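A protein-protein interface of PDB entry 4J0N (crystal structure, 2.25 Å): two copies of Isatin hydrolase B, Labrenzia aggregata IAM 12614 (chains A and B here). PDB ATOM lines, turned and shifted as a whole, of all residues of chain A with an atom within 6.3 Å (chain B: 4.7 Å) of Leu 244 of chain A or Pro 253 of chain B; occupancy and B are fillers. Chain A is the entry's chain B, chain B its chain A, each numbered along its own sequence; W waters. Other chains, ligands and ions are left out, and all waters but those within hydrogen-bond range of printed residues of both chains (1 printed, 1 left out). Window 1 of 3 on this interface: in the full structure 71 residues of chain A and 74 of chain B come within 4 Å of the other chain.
Ala 242 of chain A touches Arg 255 of chain B.
CD2 of Leu 28 of chain B touches CD1 of Leu 244 of chain A, at 3.98 Å.
Pro 253 of chain B touches Leu 244 of chain A (O to CD2, 3.4 Å).
Leu 244 of chain A touches Ile 254 of chain B.
O of Leu 244 of chain A touches NH1 of Arg 255 of chain B, at 3.9 Å.
CZ of Arg 255 of chain B touches CG of Lys 245 of chain A (3.7 Å).
Ile 246 of chain A touches Leu 28 of chain B.
Pro 253 of chain A touches Leu 244 of chain B.
Leu 244 of chain B touches Ile 254 of chain A.
The side-chain hydroxyl (OG) of Ser 252 of chain A lies within hydrogen-bond range of the backbone NH (N) of Leu 244 of chain A.
The backbone carbonyl oxygen of Thr 76 of chain B sits at hydrogen-bond distance from the backbone NH of Ile 254 of chain B.
The side-chain hydroxyl (OG1) of Thr 95 of chain A is in hydrogen-bond range of the backbone carbonyl oxygen (O) of Ile 246 of chain A (2.7 Å).
The backbone NH (N) of Leu 244 of chain B sits at hydrogen-bond distance from the side-chain hydroxyl (OG) of Ser 252 of chain B (2.9 Å).
Water W1 bridges the backbone NH (N) of Lys 245 of chain A (2.8 Å) and the backbone carbonyl oxygen (O) of Ile 254 of chain B (3.0 Å).
Leu 244 of chain A touches Pro 253 of chain B, and with the chains exchanged Pro 253 of chain A touches Leu 244 of chain B.
Leu 244 of chain A touches Ile 254 of chain B, and with the chains exchanged Ile 254 of chain A touches Leu 244 of chain B.
Positions printed for both chains: 70, 244, 252, 253 and 254.
Hydrophobic or aromatic side chains of chain B that line the printed part of chain A: Leu 28, Leu 244 and Pro 253.
Of the 12 printed residues of chain A, 8 touch a printed residue of chain B.
Printed residues of chain A that touch a printed residue of chain B: Thr 95, Ala 242, Pro 243, Leu 244, Lys 245, Ile 246, Pro 253 and Ile 254.
Hydrophobic or aromatic side chains of chain A within 4 Å of the printed part of chain B: Ala 242, Leu 244 and Pro 253.
The backbone carbonyl oxygen (O) of Lys 245 of chain A lies within hydrogen-bond range of the backbone NH (N) of Leu 28 of chain B, 2.7 Å away.
The guanidinium group (NH1) of Arg 255 of chain B sits at hydrogen-bond distance from the backbone carbonyl oxygen (O) of Pro 243 of chain A.
NH1 of Arg 255 of chain B sits at hydrogen-bond distance from O of Thr 95 of chain A (3.0 Å).
Of the printed residues of chain B, Thr 95 of chain A touches Arg 255 (3.0 Å).
Of the printed residues of chain B, Leu 244 of chain A touches Leu 28, Pro 253, Ile 254 and Arg 255.
Printed residues of chain B within 4 Å of Ile 246 of chain A: Leu 28 (3.4 Å).
Of the printed residues of chain A, Leu 28 of chain B touches Leu 244 (3.98 Å), Lys 245 (2.7 Å) and Ile 246 (3.4 Å).
Printed residues of chain A within 4 Å of Leu 244 of chain B: Pro 253 and Ile 254.
Of the printed residues of chain A, Arg 255 of chain B touches Thr 95 (3.0 Å), Ala 242 (3.8 Å), Pro 243 (3.1 Å), Leu 244 (3.9 Å) and Lys 245 (3.7 Å).
The nearest printed residue of chain B that does not touch Pro 243 of chain A is Ile 254 of chain B (5.8 Å).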
ATOM      1  N   LEU A  70      27.592 -25.697  23.194  1.00  0.00           N
ATOM      2  CA  LEU A  70      27.198 -24.557  22.369  1.00  0.00           C
ATOM      3  C   LEU A  70      25.708 -24.602  22.033  1.00  0.00           C
ATOM      4  O   LEU A  70      25.250 -25.539  21.379  1.00  0.00           O
ATOM      5  CB  LEU A  70      28.012 -24.572  21.063  1.00  0.00           C
ATOM      6  CG  LEU A  70      27.954 -23.359  20.136  1.00  0.00           C
ATOM      7  CD1 LEU A  70      28.133 -22.097  20.960  1.00  0.00           C
ATOM      8  CD2 LEU A  70      29.027 -23.440  19.029  1.00  0.00           C
ATOM      9  N   THR A  95      17.618 -25.069   9.530  1.00  0.00           N
ATOM     10  CA  THR A  95      18.944 -24.748   9.000  1.00  0.00           C
ATOM     11  C   THR A  95      19.415 -25.701   7.890  1.00  0.00           C
ATOM     12  O   THR A  95      20.168 -25.302   6.987  1.00  0.00           O
ATOM     13  CB  THR A  95      19.998 -24.662  10.128  1.00  0.00           C
ATOM     14  OG1 THR A  95      19.984 -25.874  10.902  1.00  0.00           O
ATOM     15  CG2 THR A  95      19.691 -23.472  11.029  1.00  0.00           C
ATOM     16  N   ASP A  96      18.965 -26.952   7.946  1.00  0.00           N
ATOM     17  CA  ASP A  96      19.385 -27.934   6.949  1.00  0.00           C
ATOM     18  C   ASP A  96      18.456 -28.044   5.729  1.00  0.00           C
ATOM     19  O   ASP A  96      18.718 -28.830   4.813  1.00  0.00           O
ATOM     20  CB  ASP A  96      19.627 -29.314   7.589  1.00  0.00           C
ATOM     21  CG  ASP A  96      18.388 -29.881   8.275  1.00  0.00           C
ATOM     22  OD1 ASP A  96      17.432 -29.115   8.537  1.00  0.00           O
ATOM     23  OD2 ASP A  96      18.372 -31.104   8.568  1.00  0.00           O
ATOM     24  N   ALA A 242      25.075 -17.154   6.892  1.00  0.00           N
ATOM     25  CA  ALA A 242      24.663 -18.538   6.663  1.00  0.00           C
ATOM     26  C   ALA A 242      24.849 -19.415   7.900  1.00  0.00           C
ATOM     27  O   ALA A 242      25.968 -19.538   8.433  1.00  0.00           O
ATOM     28  CB  ALA A 242      25.424 -19.121   5.494  1.00  0.00           C
ATOM     29  N   PRO A 243      23.755 -20.049   8.348  1.00  0.00           N
ATOM     30  CA  PRO A 243      23.812 -20.895   9.544  1.00  0.00           C
ATOM     31  C   PRO A 243      24.552 -22.196   9.246  1.00  0.00           C
ATOM     32  O   PRO A 243      24.563 -22.641   8.090  1.00  0.00           O
ATOM     33  CB  PRO A 243      22.336 -21.198   9.818  1.00  0.00           C
ATOM     34  CG  PRO A 243      21.692 -21.165   8.432  1.00  0.00           C
ATOM     35  CD  PRO A 243      22.430 -20.067   7.701  1.00  0.00           C
ATOM     36  N   LEU A 244      25.147 -22.806  10.270  1.00  0.00           N
ATOM     37  CA  LEU A 244      25.636 -24.173  10.141  1.00  0.00           C
ATOM     38  C   LEU A 244      24.460 -25.050   9.713  1.00  0.00           C
ATOM     39  O   LEU A 244      23.283 -24.716   9.982  1.00  0.00           O
ATOM     40  CB  LEU A 244      26.208 -24.665  11.476  1.00  0.00           C
ATOM     41  CG  LEU A 244      27.444 -23.940  12.027  1.00  0.00           C
ATOM     42  CD1 LEU A 244      27.873 -24.543  13.363  1.00  0.00           C
ATOM     43  CD2 LEU A 244      28.626 -23.943  11.031  1.00  0.00           C
ATOM     44  N   LYS A 245      24.752 -26.161   9.043  1.00  0.00           N
ATOM     45  CA  LYS A 245      23.671 -27.013   8.534  1.00  0.00           C
ATOM     46  C   LYS A 245      23.238 -28.017   9.609  1.00  0.00           C
ATOM     47  O   LYS A 245      23.338 -29.236   9.429  1.00  0.00           O
ATOM     48  CB  LYS A 245      24.088 -27.712   7.238  1.00  0.00           C
ATOM     49  CG  LYS A 245      22.929 -28.174   6.349  1.00  0.00           C
ATOM     50  CD  LYS A 245      23.441 -28.759   5.012  1.00  0.00           C
ATOM     51  CE  LYS A 245      22.277 -29.156   4.098  1.00  0.00           C
ATOM     52  NZ  LYS A 245      22.705 -29.743   2.786  1.00  0.00           N
ATOM     53  N   ILE A 246      22.750 -27.488  10.731  1.00  0.00           N
ATOM     54  CA  ILE A 246      22.389 -28.320  11.864  1.00  0.00           C
ATOM     55  C   ILE A 246      21.139 -29.104  11.514  1.00  0.00           C
ATOM     56  O   ILE A 246      20.176 -28.537  10.973  1.00  0.00           O
ATOM     57  CB  ILE A 246      22.131 -27.484  13.132  1.00  0.00           C
ATOM     58  CG1 ILE A 246      23.406 -26.748  13.539  1.00  0.00           C
ATOM     59  CG2 ILE A 246      21.653 -28.376  14.285  1.00  0.00           C
ATOM     60  CD1 ILE A 246      23.205 -25.774  14.685  1.00  0.00           C
ATOM     61  N   GLY A 251      18.362 -22.722  14.428  1.00  0.00           N
ATOM     62  CA  GLY A 251      19.268 -21.592  14.384  1.00  0.00           C
ATOM     63  C   GLY A 251      20.714 -22.057  14.477  1.00  0.00           C
ATOM     64  O   GLY A 251      20.980 -23.263  14.513  1.00  0.00           O
ATOM     65  N   SER A 252      21.646 -21.107  14.519  1.00  0.00           N
ATOM     66  CA  SER A 252      23.072 -21.428  14.640  1.00  0.00           C
ATOM     67  C   SER A 252      23.903 -20.175  14.833  1.00  0.00           C
ATOM     68  O   SER A 252      23.571 -19.118  14.288  1.00  0.00           O
ATOM     69  CB  SER A 252      23.578 -22.158  13.386  1.00  0.00           C
ATOM     70  OG  SER A 252      24.978 -21.968  13.207  1.00  0.00           O
ATOM     71  N   PRO A 253      25.001 -20.293  15.590  1.00  0.00           N
ATOM     72  CA  PRO A 253      25.997 -19.222  15.505  1.00  0.00           C
ATOM     73  C   PRO A 253      26.487 -19.144  14.058  1.00  0.00           C
ATOM     74  O   PRO A 253      26.443 -20.148  13.339  1.00  0.00           O
ATOM     75  CB  PRO A 253      27.134 -19.723  16.410  1.00  0.00           C
ATOM     76  CG  PRO A 253      26.964 -21.231  16.440  1.00  0.00           C
ATOM     77  CD  PRO A 253      25.472 -21.448  16.378  1.00  0.00           C
ATOM     78  N   ILE A 254      26.920 -17.962  13.631  1.00  0.00           N
ATOM     79  CA  ILE A 254      27.359 -17.757  12.263  1.00  0.00           C
ATOM     80  C   ILE A 254      28.602 -16.898  12.259  1.00  0.00           C
ATOM     81  O   ILE A 254      28.912 -16.238  13.262  1.00  0.00           O
ATOM     82  CB  ILE A 254      26.310 -16.996  11.451  1.00  0.00           C
ATOM     83  CG1 ILE A 254      25.983 -15.678  12.163  1.00  0.00           C
ATOM     84  CG2 ILE A 254      25.054 -17.865  11.220  1.00  0.00           C
ATOM     85  CD1 ILE A 254      25.318 -14.641  11.292  1.00  0.00           C
ATOM     86  N   LEU B  28      24.934 -31.409   9.686  1.00  0.00           N
ATOM     87  CA  LEU B  28      25.622 -31.442  10.971  1.00  0.00           C
ATOM     88  C   LEU B  28      24.709 -32.021  12.050  1.00  0.00           C
ATOM     89  O   LEU B  28      23.772 -31.355  12.522  1.00  0.00           O
ATOM     90  CB  LEU B  28      26.068 -30.028  11.351  1.00  0.00           C
ATOM     91  CG  LEU B  28      26.973 -29.890  12.580  1.00  0.00           C
ATOM     92  CD1 LEU B  28      28.197 -30.814  12.461  1.00  0.00           C
ATOM     93  CD2 LEU B  28      27.415 -28.450  12.726  1.00  0.00           C
ATOM     94  N   LEU B  70      29.701 -30.172  20.565  1.00  0.00           N
ATOM     95  CA  LEU B  70      30.238 -29.941  19.220  1.00  0.00           C
ATOM     96  C   LEU B  70      31.756 -29.737  19.189  1.00  0.00           C
ATOM     97  O   LEU B  70      32.266 -28.765  19.746  1.00  0.00           O
ATOM     98  CB  LEU B  70      29.553 -28.710  18.609  1.00  0.00           C
ATOM     99  CG  LEU B  70      29.795 -28.394  17.137  1.00  0.00           C
ATOM    100  CD1 LEU B  70      29.709 -29.671  16.319  1.00  0.00           C
ATOM    101  CD2 LEU B  70      28.763 -27.377  16.641  1.00  0.00           C
ATOM    102  N   GLY B  71      32.471 -30.633  18.511  1.00  0.00           N
ATOM    103  CA  GLY B  71      33.900 -30.454  18.301  1.00  0.00           C
ATOM    104  C   GLY B  71      34.156 -29.363  17.272  1.00  0.00           C
ATOM    105  O   GLY B  71      33.347 -29.161  16.351  1.00  0.00           O
ATOM    106  N   GLU B  72      35.272 -28.650  17.422  1.00  0.00           N
ATOM    107  CA  GLU B  72      35.674 -27.649  16.435  1.00  0.00           C
ATOM    108  C   GLU B  72      35.742 -28.306  15.058  1.00  0.00           C
ATOM    109  O   GLU B  72      35.259 -27.765  14.058  1.00  0.00           O
ATOM    110  CB  GLU B  72      37.053 -27.068  16.796  1.00  0.00           C
ATOM    111  CG  GLU B  72      37.081 -26.123  17.994  1.00  0.00           C
ATOM    112  CD  GLU B  72      38.493 -25.641  18.312  1.00  0.00           C
ATOM    113  OE1 GLU B  72      39.454 -26.374  17.965  1.00  0.00           O
ATOM    114  OE2 GLU B  72      38.649 -24.535  18.905  1.00  0.00           O
ATOM    115  N   SER B  74      34.247 -30.724  13.087  1.00  0.00           N
ATOM    116  CA  SER B  74      33.059 -31.562  12.939  1.00  0.00           C
ATOM    117  C   SER B  74      32.363 -31.291  11.610  1.00  0.00           C
ATOM    118  O   SER B  74      31.996 -30.141  11.306  1.00  0.00           O
ATOM    119  CB  SER B  74      32.077 -31.304  14.102  1.00  0.00           C
ATOM    120  OG  SER B  74      32.708 -31.473  15.366  1.00  0.00           O
ATOM    121  N   THR B  76      31.542 -30.649   7.709  1.00  0.00           N
ATOM    122  CA  THR B  76      32.181 -29.654   6.853  1.00  0.00           C
ATOM    123  C   THR B  76      32.799 -28.573   7.744  1.00  0.00           C
ATOM    124  O   THR B  76      32.084 -27.835   8.440  1.00  0.00           O
ATOM    125  CB  THR B  76      31.185 -29.028   5.883  1.00  0.00           C
ATOM    126  OG1 THR B  76      30.425 -30.073   5.269  1.00  0.00           O
ATOM    127  CG2 THR B  76      31.928 -28.239   4.799  1.00  0.00           C
ATOM    128  N   HIS B  77      34.128 -28.487   7.730  1.00  0.00           N
ATOM    129  CA  HIS B  77      34.823 -27.632   8.685  1.00  0.00           C
ATOM    130  C   HIS B  77      36.141 -27.006   8.184  1.00  0.00           C
ATOM    131  O   HIS B  77      36.744 -27.462   7.202  1.00  0.00           O
ATOM    132  CB  HIS B  77      35.014 -28.379  10.024  1.00  0.00           C
ATOM    133  CG  HIS B  77      36.144 -29.371  10.021  1.00  0.00           C
ATOM    134  ND1 HIS B  77      35.956 -30.710   9.707  1.00  0.00           N
ATOM    135  CD2 HIS B  77      37.451 -29.231  10.313  1.00  0.00           C
ATOM    136  CE1 HIS B  77      37.110 -31.333   9.796  1.00  0.00           C
ATOM    137  NE2 HIS B  77      38.044 -30.475  10.165  1.00  0.00           N
ATOM    138  N   LEU B 244      33.427 -19.929  12.414  1.00  0.00           N
ATOM    139  CA  LEU B 244      32.945 -19.261  13.619  1.00  0.00           C
ATOM    140  C   LEU B 244      34.102 -18.566  14.342  1.00  0.00           C
ATOM    141  O   LEU B 244      35.252 -19.048  14.358  1.00  0.00           O
ATOM    142  CB  LEU B 244      32.283 -20.270  14.563  1.00  0.00           C
ATOM    143  CG  LEU B 244      31.096 -21.031  13.979  1.00  0.00           C
ATOM    144  CD1 LEU B 244      30.495 -21.943  15.043  1.00  0.00           C
ATOM    145  CD2 LEU B 244      30.045 -20.073  13.422  1.00  0.00           C
ATOM    146  N   SER B 252      36.709 -24.771  12.956  1.00  0.00           N
ATOM    147  CA  SER B 252      35.273 -24.557  13.173  1.00  0.00           C
ATOM    148  C   SER B 252      34.432 -25.279  12.126  1.00  0.00           C
ATOM    149  O   SER B 252      34.816 -25.339  10.953  1.00  0.00           O
ATOM    150  CB  SER B 252      34.957 -23.056  13.150  1.00  0.00           C
ATOM    151  OG  SER B 252      33.566 -22.796  12.994  1.00  0.00           O
ATOM    152  N   PRO B 253      33.272 -25.827  12.540  1.00  0.00           N
ATOM    153  CA  PRO B 253      32.325 -26.199  11.480  1.00  0.00           C
ATOM    154  C   PRO B 253      31.962 -24.942  10.678  1.00  0.00           C
ATOM    155  O   PRO B 253      31.977 -23.839  11.231  1.00  0.00           O
ATOM    156  CB  PRO B 253      31.098 -26.715  12.256  1.00  0.00           C
ATOM    157  CG  PRO B 253      31.235 -26.124  13.638  1.00  0.00           C
ATOM    158  CD  PRO B 253      32.723 -26.058  13.891  1.00  0.00           C
ATOM    159  N   ILE B 254      31.688 -25.104   9.387  1.00  0.00           N
ATOM    160  CA  ILE B 254      31.355 -23.982   8.536  1.00  0.00           C
ATOM    161  C   ILE B 254      30.131 -24.288   7.700  1.00  0.00           C
ATOM    162  O   ILE B 254      29.749 -25.458   7.541  1.00  0.00           O
ATOM    163  CB  ILE B 254      32.509 -23.640   7.587  1.00  0.00           C
ATOM    164  CG1 ILE B 254      32.901 -24.871   6.775  1.00  0.00           C
ATOM    165  CG2 ILE B 254      33.691 -23.123   8.371  1.00  0.00           C
ATOM    166  CD1 ILE B 254      33.892 -24.557   5.657  1.00  0.00           C
ATOM    167  N   ARG B 255      29.507 -23.230   7.183  1.00  0.00           N
ATOM    168  CA  ARG B 255      28.523 -23.389   6.118  1.00  0.00           C
ATOM    169  C   ARG B 255      29.167 -22.941   4.813  1.00  0.00           C
ATOM    170  O   ARG B 255      28.929 -21.821   4.339  1.00  0.00           O
ATOM    171  CB  ARG B 255      27.251 -22.567   6.388  1.00  0.00           C
ATOM    172  CG  ARG B 255      26.114 -22.878   5.412  1.00  0.00           C
ATOM    173  CD  ARG B 255      25.619 -24.299   5.619  1.00  0.00           C
ATOM    174  NE  ARG B 255      24.565 -24.721   4.692  1.00  0.00           N
ATOM    175  CZ  ARG B 255      23.258 -24.712   4.965  1.00  0.00           C
ATOM    176  NH1 ARG B 255      22.802 -24.272   6.135  1.00  0.00           N
ATOM    177  NH2 ARG B 255      22.403 -25.150   4.061  1.00  0.00           N
HETATM  178  O   HOH W   1      27.495 -26.835   8.913  1.00  0.00           O
